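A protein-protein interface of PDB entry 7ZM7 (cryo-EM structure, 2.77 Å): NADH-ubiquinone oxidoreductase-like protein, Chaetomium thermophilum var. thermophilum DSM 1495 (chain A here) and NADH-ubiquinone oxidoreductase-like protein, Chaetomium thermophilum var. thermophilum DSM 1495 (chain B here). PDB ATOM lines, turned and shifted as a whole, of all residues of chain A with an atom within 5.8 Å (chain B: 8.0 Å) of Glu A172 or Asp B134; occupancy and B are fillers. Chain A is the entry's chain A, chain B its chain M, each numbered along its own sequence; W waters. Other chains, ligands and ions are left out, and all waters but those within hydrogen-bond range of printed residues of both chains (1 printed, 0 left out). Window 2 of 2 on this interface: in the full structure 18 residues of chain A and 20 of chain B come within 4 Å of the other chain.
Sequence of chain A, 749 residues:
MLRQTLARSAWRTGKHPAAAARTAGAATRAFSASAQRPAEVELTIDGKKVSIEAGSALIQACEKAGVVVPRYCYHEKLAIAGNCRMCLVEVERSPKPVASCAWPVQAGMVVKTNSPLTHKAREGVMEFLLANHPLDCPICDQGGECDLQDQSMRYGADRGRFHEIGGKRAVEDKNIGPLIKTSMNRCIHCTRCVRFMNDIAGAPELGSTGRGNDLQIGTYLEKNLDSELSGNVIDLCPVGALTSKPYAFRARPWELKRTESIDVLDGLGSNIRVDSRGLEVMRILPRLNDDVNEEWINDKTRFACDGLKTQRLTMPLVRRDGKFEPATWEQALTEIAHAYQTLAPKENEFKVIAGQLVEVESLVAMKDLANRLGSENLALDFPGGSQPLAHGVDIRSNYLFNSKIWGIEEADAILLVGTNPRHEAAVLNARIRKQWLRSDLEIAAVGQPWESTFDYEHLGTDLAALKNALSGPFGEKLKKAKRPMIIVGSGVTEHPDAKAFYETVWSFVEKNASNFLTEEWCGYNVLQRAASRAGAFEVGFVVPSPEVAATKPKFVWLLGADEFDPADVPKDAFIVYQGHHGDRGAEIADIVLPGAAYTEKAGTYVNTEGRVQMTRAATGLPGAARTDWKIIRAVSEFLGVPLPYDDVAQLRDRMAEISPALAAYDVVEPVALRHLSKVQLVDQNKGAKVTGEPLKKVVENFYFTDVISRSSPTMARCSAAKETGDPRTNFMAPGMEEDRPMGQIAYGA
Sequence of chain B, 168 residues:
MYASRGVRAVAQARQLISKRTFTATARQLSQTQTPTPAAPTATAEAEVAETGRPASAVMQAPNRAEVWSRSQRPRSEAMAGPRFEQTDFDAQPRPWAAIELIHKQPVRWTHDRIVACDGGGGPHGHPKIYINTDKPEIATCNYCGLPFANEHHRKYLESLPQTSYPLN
The backbone carbonyl oxygen (O) of Asp A173 sits at hydrogen-bond distance from the side-chain amino group (NZ) of Lys B135 (2.6 Å).
The backbone carbonyl oxygen (O) of Ala A170 lies within hydrogen-bond range of the side-chain amide nitrogen (ND2) of Asn B132, at 3.3 Å.
The backbone NH (N) of Glu A172 sits close to the side-chain amide oxygen (OD1) of Asn B132 (3.4 Å).
OD1 of Asn A185 is in hydrogen-bond range of N of Val A171 (2.7 Å).
A ring nitrogen (NE2) of His B153 lies close to the backbone carbonyl oxygen of Lys B135 (3.1 Å).
The side-chain carboxylate of Asp A173 is in hydrogen-bond range of the backbone NH of Met A184, at 3.3 Å.
A ring nitrogen (NE2) of His B153 sits at hydrogen-bond distance from the backbone carbonyl oxygen of Asp B134 (3.5 Å).
The guanidinium group of Arg B113 is in salt-bridge range of the side-chain carboxylate of Asp B134.
OD2 of Asp B134 is in hydrogen-bond range of ND2 of Asn B132.
Ile B114 touches Ala A170.
CB of Asn B132 touches C of Val A171, at 3.7 Å.
Asp B134 touches Glu A172.
Lys B135 touches Glu A172 (CE to OE2, 3.5 Å).
Asp B134 touches just one residue of chain A: Glu A172 (3.8 Å).
Printed residues of chain A within 4 Å of Lys B135: Glu A172 and Asp A173.
Printed residues of chain B within 4 Å of Asp A173: Lys B135.
Printed residues of chain B within 4 Å of Val A171: Asn B132.
Asn B150 touches none of the printed residues of chain A.
The nearest residue of chain B that does not touch Glu A172 is Thr B133 (6.4 Å).
The nearest printed residue of chain A that does not touch Ile B114 is Val A171 (5.8 Å).
Of the 9 printed residues of chain A, 4 touch a printed residue of chain B.
Hydrophobic or aromatic side chains of chain A within 4 Å of the printed part of chain B: Ala A170.
Hydrophobic or aromatic side chains of chain B that line the printed part of chain A: Ile B114.
Among the printed residues, 7 pairs touch across the chains.
Among the printed residues, no Asp or Glu carboxylate lies within 4 Å of a Lys or Arg side-chain nitrogen of the other chain.
Water W1 lies within hydrogen-bond range of O of Val A171 and N of Asn B132.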
ATOM      1  N   ALA A 170       5.083   4.872  -0.645  1.00  0.00           N
ATOM      2  CA  ALA A 170       3.808   5.531  -0.413  1.00  0.00           C
ATOM      3  C   ALA A 170       3.040   4.737   0.621  1.00  0.00           C
ATOM      4  O   ALA A 170       3.047   3.508   0.589  1.00  0.00           O
ATOM      5  CB  ALA A 170       2.980   5.665  -1.688  1.00  0.00           C
ATOM      6  N   VAL A 171       2.399   5.435   1.547  1.00  0.00           N
ATOM      7  CA  VAL A 171       1.689   4.792   2.638  1.00  0.00           C
ATOM      8  C   VAL A 171       0.283   5.357   2.721  1.00  0.00           C
ATOM      9  O   VAL A 171       0.028   6.509   2.360  1.00  0.00           O
ATOM     10  CB  VAL A 171       2.425   4.941   3.993  1.00  0.00           C
ATOM     11  CG1 VAL A 171       3.728   4.210   3.983  1.00  0.00           C
ATOM     12  CG2 VAL A 171       2.675   6.386   4.299  1.00  0.00           C
ATOM     13  N   GLU A 172      -0.635   4.532   3.204  1.00  0.00           N
ATOM     14  CA  GLU A 172      -2.009   4.969   3.368  1.00  0.00           C
ATOM     15  C   GLU A 172      -2.135   5.938   4.538  1.00  0.00           C
ATOM     16  O   GLU A 172      -1.321   5.944   5.463  1.00  0.00           O
ATOM     17  CB  GLU A 172      -2.916   3.772   3.589  1.00  0.00           C
ATOM     18  CG  GLU A 172      -2.942   3.290   5.000  1.00  0.00           C
ATOM     19  CD  GLU A 172      -3.745   2.037   5.120  1.00  0.00           C
ATOM     20  OE1 GLU A 172      -3.790   1.281   4.128  1.00  0.00           O
ATOM     21  OE2 GLU A 172      -4.346   1.807   6.189  1.00  0.00           O
ATOM     22  N   ASP A 173      -3.216   6.719   4.507  1.00  0.00           N
ATOM     23  CA  ASP A 173      -3.453   7.714   5.579  1.00  0.00           C
ATOM     24  C   ASP A 173      -4.071   7.026   6.786  1.00  0.00           C
ATOM     25  O   ASP A 173      -4.458   5.862   6.670  1.00  0.00           O
ATOM     26  CB  ASP A 173      -4.249   8.913   5.070  1.00  0.00           C
ATOM     27  CG  ASP A 173      -3.383   9.929   4.339  1.00  0.00           C
ATOM     28  OD1 ASP A 173      -2.149   9.877   4.505  1.00  0.00           O
ATOM     29  OD2 ASP A 173      -3.947  10.762   3.609  1.00  0.00           O
ATOM     30  N   LYS A 174      -4.098   7.705   7.924  1.00  0.00           N
ATOM     31  CA  LYS A 174      -4.584   7.039   9.151  1.00  0.00           C
ATOM     32  C   LYS A 174      -5.614   7.932   9.836  1.00  0.00           C
ATOM     33  O   LYS A 174      -5.418   9.148   9.868  1.00  0.00           O
ATOM     34  CB  LYS A 174      -3.394   6.661  10.034  1.00  0.00           C
ATOM     35  CG  LYS A 174      -2.540   5.506   9.533  1.00  0.00           C
ATOM     36  CD  LYS A 174      -1.111   5.904   9.273  1.00  0.00           C
ATOM     37  CE  LYS A 174      -0.270   4.785   8.704  1.00  0.00           C
ATOM     38  NZ  LYS A 174       1.085   5.262   8.338  1.00  0.00           N
ATOM     39  N   MET A 184       0.683  10.921   5.935  1.00  0.00           N
ATOM     40  CA  MET A 184       1.831  10.134   6.464  1.00  0.00           C
ATOM     41  C   MET A 184       2.972   9.894   5.476  1.00  0.00           C
ATOM     42  O   MET A 184       4.054   9.536   5.954  1.00  0.00           O
ATOM     43  CB  MET A 184       1.360   8.813   7.073  1.00  0.00           C
ATOM     44  CG  MET A 184       0.404   9.017   8.232  1.00  0.00           C
ATOM     45  SD  MET A 184       1.041  10.162   9.484  1.00  0.00           S
ATOM     46  CE  MET A 184       2.387   9.201  10.173  1.00  0.00           C
ATOM     47  N   ASN A 185       2.760  10.056   4.172  1.00  0.00           N
ATOM     48  CA  ASN A 185       3.915   9.933   3.290  1.00  0.00           C
ATOM     49  C   ASN A 185       5.040  10.835   3.724  1.00  0.00           C
ATOM     50  O   ASN A 185       6.190  10.600   3.360  1.00  0.00           O
ATOM     51  CB  ASN A 185       3.573  10.300   1.852  1.00  0.00           C
ATOM     52  CG  ASN A 185       2.994   9.173   1.093  1.00  0.00           C
ATOM     53  OD1 ASN A 185       2.792   8.098   1.623  1.00  0.00           O
ATOM     54  ND2 ASN A 185       2.710   9.407  -0.163  1.00  0.00           N
ATOM     55  N   GLN A 216       5.587   2.472  10.142  1.00  0.00           N
ATOM     56  CA  GLN A 216       4.521   3.456  10.062  1.00  0.00           C
ATOM     57  C   GLN A 216       4.127   3.934  11.447  1.00  0.00           C
ATOM     58  O   GLN A 216       4.190   3.183  12.416  1.00  0.00           O
ATOM     59  CB  GLN A 216       3.314   2.880   9.336  1.00  0.00           C
ATOM     60  CG  GLN A 216       3.652   2.516   7.927  1.00  0.00           C
ATOM     61  CD  GLN A 216       2.609   1.688   7.261  1.00  0.00           C
ATOM     62  OE1 GLN A 216       1.518   1.515   7.779  1.00  0.00           O
ATOM     63  NE2 GLN A 216       2.945   1.143   6.112  1.00  0.00           N
ATOM     64  N   GLU A 222      -7.695   1.748  13.941  1.00  0.00           N
ATOM     65  CA  GLU A 222      -8.032   3.193  13.948  1.00  0.00           C
ATOM     66  C   GLU A 222      -8.737   3.563  15.242  1.00  0.00           C
ATOM     67  O   GLU A 222      -9.762   2.942  15.559  1.00  0.00           O
ATOM     68  CB  GLU A 222      -8.892   3.565  12.743  1.00  0.00           C
ATOM     69  CG  GLU A 222      -8.084   3.788  11.481  1.00  0.00           C
ATOM     70  CD  GLU A 222      -8.864   3.552  10.201  1.00  0.00           C
ATOM     71  OE1 GLU A 222     -10.105   3.622  10.247  1.00  0.00           O
ATOM     72  OE2 GLU A 222      -8.227   3.280   9.165  1.00  0.00           O
ATOM     73  N   HIS B 111      -2.932  -2.936 -10.568  1.00  0.00           N
ATOM     74  CA  HIS B 111      -2.530  -4.112  -9.824  1.00  0.00           C
ATOM     75  C   HIS B 111      -1.462  -3.814  -8.791  1.00  0.00           C
ATOM     76  O   HIS B 111      -0.986  -4.738  -8.127  1.00  0.00           O
ATOM     77  CB  HIS B 111      -2.021  -5.185 -10.783  1.00  0.00           C
ATOM     78  CG  HIS B 111      -3.082  -5.750 -11.671  1.00  0.00           C
ATOM     79  ND1 HIS B 111      -3.764  -6.909 -11.369  1.00  0.00           N
ATOM     80  CD2 HIS B 111      -3.583  -5.314 -12.850  1.00  0.00           C
ATOM     81  CE1 HIS B 111      -4.637  -7.164 -12.327  1.00  0.00           C
ATOM     82  NE2 HIS B 111      -4.548  -6.211 -13.237  1.00  0.00           N
ATOM     83  N   ASP B 112      -1.077  -2.559  -8.638  1.00  0.00           N
ATOM     84  CA  ASP B 112       0.061  -2.190  -7.822  1.00  0.00           C
ATOM     85  C   ASP B 112      -0.389  -1.491  -6.553  1.00  0.00           C
ATOM     86  O   ASP B 112      -1.444  -0.863  -6.510  1.00  0.00           O
ATOM     87  CB  ASP B 112       1.018  -1.286  -8.599  1.00  0.00           C
ATOM     88  CG  ASP B 112       1.729  -2.015  -9.706  1.00  0.00           C
ATOM     89  OD1 ASP B 112       1.739  -3.262  -9.684  1.00  0.00           O
ATOM     90  OD2 ASP B 112       2.292  -1.343 -10.591  1.00  0.00           O
ATOM     91  N   ARG B 113       0.438  -1.602  -5.517  1.00  0.00           N
ATOM     92  CA  ARG B 113       0.146  -0.904  -4.274  1.00  0.00           C
ATOM     93  C   ARG B 113       0.388   0.587  -4.410  1.00  0.00           C
ATOM     94  O   ARG B 113      -0.405   1.395  -3.920  1.00  0.00           O
ATOM     95  CB  ARG B 113       0.983  -1.484  -3.142  1.00  0.00           C
ATOM     96  CG  ARG B 113       1.080  -2.990  -3.177  1.00  0.00           C
ATOM     97  CD  ARG B 113       1.643  -3.520  -1.881  1.00  0.00           C
ATOM     98  NE  ARG B 113       0.999  -2.898  -0.734  1.00  0.00           N
ATOM     99  CZ  ARG B 113       1.604  -2.692   0.426  1.00  0.00           C
ATOM    100  NH1 ARG B 113       0.959  -2.110   1.423  1.00  0.00           N
ATOM    101  NH2 ARG B 113       2.861  -3.068   0.583  1.00  0.00           N
ATOM    102  N   ILE B 114       1.470   0.973  -5.071  1.00  0.00           N
ATOM    103  CA  ILE B 114       1.828   2.368  -5.249  1.00  0.00           C
ATOM    104  C   ILE B 114       1.784   2.684  -6.731  1.00  0.00           C
ATOM    105  O   ILE B 114       2.390   1.978  -7.537  1.00  0.00           O
ATOM    106  CB  ILE B 114       3.213   2.672  -4.664  1.00  0.00           C
ATOM    107  CG1 ILE B 114       3.266   2.243  -3.202  1.00  0.00           C
ATOM    108  CG2 ILE B 114       3.536   4.148  -4.836  1.00  0.00           C
ATOM    109  CD1 ILE B 114       4.585   1.728  -2.805  1.00  0.00           C
ATOM    110  N   ILE B 131       0.822   7.445  -4.914  1.00  0.00           N
ATOM    111  CA  ILE B 131      -0.442   7.198  -4.239  1.00  0.00           C
ATOM    112  C   ILE B 131      -0.510   5.731  -3.855  1.00  0.00           C
ATOM    113  O   ILE B 131      -0.231   4.852  -4.672  1.00  0.00           O
ATOM    114  CB  ILE B 131      -1.645   7.615  -5.107  1.00  0.00           C
ATOM    115  CG1 ILE B 131      -1.671   9.131  -5.359  1.00  0.00           C
ATOM    116  CG2 ILE B 131      -2.919   7.158  -4.495  1.00  0.00           C
ATOM    117  CD1 ILE B 131      -0.937   9.622  -6.562  1.00  0.00           C
ATOM    118  N   ASN B 132      -0.871   5.475  -2.605  1.00  0.00           N
ATOM    119  CA  ASN B 132      -1.025   4.132  -2.073  1.00  0.00           C
ATOM    120  C   ASN B 132      -2.488   3.725  -2.157  1.00  0.00           C
ATOM    121  O   ASN B 132      -3.371   4.472  -1.737  1.00  0.00           O
ATOM    122  CB  ASN B 132      -0.536   4.087  -0.627  1.00  0.00           C
ATOM    123  CG  ASN B 132      -0.702   2.738   0.001  1.00  0.00           C
ATOM    124  OD1 ASN B 132      -1.686   2.487   0.677  1.00  0.00           O
ATOM    125  ND2 ASN B 132       0.274   1.870  -0.184  1.00  0.00           N
ATOM    126  N   THR B 133      -2.744   2.555  -2.718  1.00  0.00           N
ATOM    127  CA  THR B 133      -4.104   2.093  -2.941  1.00  0.00           C
ATOM    128  C   THR B 133      -4.266   0.787  -2.188  1.00  0.00           C
ATOM    129  O   THR B 133      -4.400  -0.271  -2.792  1.00  0.00           O
ATOM    130  CB  THR B 133      -4.356   1.909  -4.419  1.00  0.00           C
ATOM    131  OG1 THR B 133      -3.449   0.937  -4.932  1.00  0.00           O
ATOM    132  CG2 THR B 133      -4.124   3.200  -5.163  1.00  0.00           C
ATOM    133  N   ASP B 134      -4.307   0.867  -0.865  1.00  0.00           N
ATOM    134  CA  ASP B 134      -4.415  -0.343  -0.066  1.00  0.00           C
ATOM    135  C   ASP B 134      -5.658  -0.311   0.792  1.00  0.00           C
ATOM    136  O   ASP B 134      -6.073  -1.339   1.322  1.00  0.00           O
ATOM    137  CB  ASP B 134      -3.199  -0.547   0.822  1.00  0.00           C
ATOM    138  CG  ASP B 134      -2.014  -1.023   0.064  1.00  0.00           C
ATOM    139  OD1 ASP B 134      -2.203  -1.619  -1.011  1.00  0.00           O
ATOM    140  OD2 ASP B 134      -0.886  -0.843   0.560  1.00  0.00           O
ATOM    141  N   LYS B 135      -6.244   0.855   0.956  1.00  0.00           N
ATOM    142  CA  LYS B 135      -7.538   0.906   1.585  1.00  0.00           C
ATOM    143  C   LYS B 135      -8.608   0.493   0.588  1.00  0.00           C
ATOM    144  O   LYS B 135      -8.489   0.760  -0.606  1.00  0.00           O
ATOM    145  CB  LYS B 135      -7.820   2.301   2.103  1.00  0.00           C
ATOM    146  CG  LYS B 135      -6.943   2.643   3.246  1.00  0.00           C
ATOM    147  CD  LYS B 135      -7.245   4.009   3.720  1.00  0.00           C
ATOM    148  CE  LYS B 135      -6.443   4.306   4.932  1.00  0.00           C
ATOM    149  NZ  LYS B 135      -6.733   5.673   5.425  1.00  0.00           N
ATOM    150  N   PRO B 136      -9.673  -0.142   1.051  1.00  0.00           N
ATOM    151  CA  PRO B 136     -10.776  -0.502   0.147  1.00  0.00           C
ATOM    152  C   PRO B 136     -11.630   0.710  -0.208  1.00  0.00           C
ATOM    153  O   PRO B 136     -12.835   0.750   0.031  1.00  0.00           O
ATOM    154  CB  PRO B 136     -11.542  -1.546   0.962  1.00  0.00           C
ATOM    155  CG  PRO B 136     -11.010  -1.467   2.368  1.00  0.00           C
ATOM    156  CD  PRO B 136     -10.005  -0.391   2.457  1.00  0.00           C
ATOM    157  N   GLU B 137     -10.985   1.727  -0.769  1.00  0.00           N
ATOM    158  CA  GLU B 137     -11.653   2.938  -1.201  1.00  0.00           C
ATOM    159  C   GLU B 137     -11.026   3.345  -2.519  1.00  0.00           C
ATOM    160  O   GLU B 137     -10.168   2.644  -3.053  1.00  0.00           O
ATOM    161  CB  GLU B 137     -11.542   4.044  -0.145  1.00  0.00           C
ATOM    162  CG  GLU B 137     -10.134   4.550   0.090  1.00  0.00           C
ATOM    163  CD  GLU B 137     -10.060   5.594   1.188  1.00  0.00           C
ATOM    164  OE1 GLU B 137     -11.110   5.911   1.784  1.00  0.00           O
ATOM    165  OE2 GLU B 137      -8.947   6.094   1.462  1.00  0.00           O
ATOM    166  N   ALA B 139      -8.536   5.959  -4.110  1.00  0.00           N
ATOM    167  CA  ALA B 139      -7.483   6.910  -3.793  1.00  0.00           C
ATOM    168  C   ALA B 139      -7.373   7.969  -4.878  1.00  0.00           C
ATOM    169  O   ALA B 139      -7.452   7.658  -6.064  1.00  0.00           O
ATOM    170  CB  ALA B 139      -6.154   6.178  -3.644  1.00  0.00           C
ATOM    171  N   PHE B 148      -7.800   6.555  -8.512  1.00  0.00           N
ATOM    172  CA  PHE B 148      -7.038   5.320  -8.602  1.00  0.00           C
ATOM    173  C   PHE B 148      -7.642   4.333  -7.628  1.00  0.00           C
ATOM    174  O   PHE B 148      -8.135   4.726  -6.572  1.00  0.00           O
ATOM    175  CB  PHE B 148      -5.558   5.530  -8.276  1.00  0.00           C
ATOM    176  CG  PHE B 148      -4.878   6.485  -9.193  1.00  0.00           C
ATOM    177  CD1 PHE B 148      -4.910   7.839  -8.946  1.00  0.00           C
ATOM    178  CD2 PHE B 148      -4.246   6.038 -10.315  1.00  0.00           C
ATOM    179  CE1 PHE B 148      -4.310   8.714  -9.796  1.00  0.00           C
ATOM    180  CE2 PHE B 148      -3.639   6.908 -11.159  1.00  0.00           C
ATOM    181  CZ  PHE B 148      -3.668   8.244 -10.904  1.00  0.00           C
ATOM    182  N   ALA B 149      -7.633   3.059  -7.991  1.00  0.00           N
ATOM    183  CA  ALA B 149      -8.164   2.031  -7.116  1.00  0.00           C
ATOM    184  C   ALA B 149      -7.488   0.718  -7.447  1.00  0.00           C
ATOM    185  O   ALA B 149      -7.255   0.408  -8.616  1.00  0.00           O
ATOM    186  CB  ALA B 149      -9.683   1.890  -7.240  1.00  0.00           C
ATOM    187  N   ASN B 150      -7.156  -0.038  -6.413  1.00  0.00           N
ATOM    188  CA  ASN B 150      -6.528  -1.325  -6.617  1.00  0.00           C
ATOM    189  C   ASN B 150      -7.553  -2.333  -7.104  1.00  0.00           C
ATOM    190  O   ASN B 150      -8.721  -2.306  -6.712  1.00  0.00           O
ATOM    191  CB  ASN B 150      -5.878  -1.817  -5.333  1.00  0.00           C
ATOM    192  CG  ASN B 150      -4.717  -2.736  -5.594  1.00  0.00           C
ATOM    193  OD1 ASN B 150      -4.865  -3.791  -6.201  1.00  0.00           O
ATOM    194  ND2 ASN B 150      -3.542  -2.330  -5.148  1.00  0.00           N
ATOM    195  N   HIS B 152      -7.870  -5.247  -6.284  1.00  0.00           N
ATOM    196  CA  HIS B 152      -8.341  -6.104  -5.208  1.00  0.00           C
ATOM    197  C   HIS B 152      -9.635  -5.618  -4.591  1.00  0.00           C
ATOM    198  O   HIS B 152     -10.363  -6.425  -4.005  1.00  0.00           O
ATOM    199  CB  HIS B 152      -7.279  -6.223  -4.122  1.00  0.00           C
ATOM    200  CG  HIS B 152      -6.342  -7.370  -4.323  1.00  0.00           C
ATOM    201  ND1 HIS B 152      -5.236  -7.294  -5.141  1.00  0.00           N
ATOM    202  CD2 HIS B 152      -6.349  -8.626  -3.818  1.00  0.00           C
ATOM    203  CE1 HIS B 152      -4.601  -8.451  -5.129  1.00  0.00           C
ATOM    204  NE2 HIS B 152      -5.256  -9.277  -4.333  1.00  0.00           N
ATOM    205  N   HIS B 153      -9.944  -4.329  -4.692  1.00  0.00           N
ATOM    206  CA  HIS B 153     -11.144  -3.777  -4.084  1.00  0.00           C
ATOM    207  C   HIS B 153     -12.262  -3.582  -5.087  1.00  0.00           C
ATOM    208  O   HIS B 153     -13.243  -2.901  -4.781  1.00  0.00           O
ATOM    209  CB  HIS B 153     -10.841  -2.454  -3.390  1.00  0.00           C
ATOM    210  CG  HIS B 153      -9.553  -2.447  -2.635  1.00  0.00           C
ATOM    211  ND1 HIS B 153      -9.164  -3.484  -1.820  1.00  0.00           N
ATOM    212  CD2 HIS B 153      -8.564  -1.526  -2.575  1.00  0.00           C
ATOM    213  CE1 HIS B 153      -7.991  -3.200  -1.287  1.00  0.00           C
ATOM    214  NE2 HIS B 153      -7.605  -2.019  -1.730  1.00  0.00           N
HETATM  215  O   HOH W   1      -0.485   7.494  -0.274  1.00  0.00           O
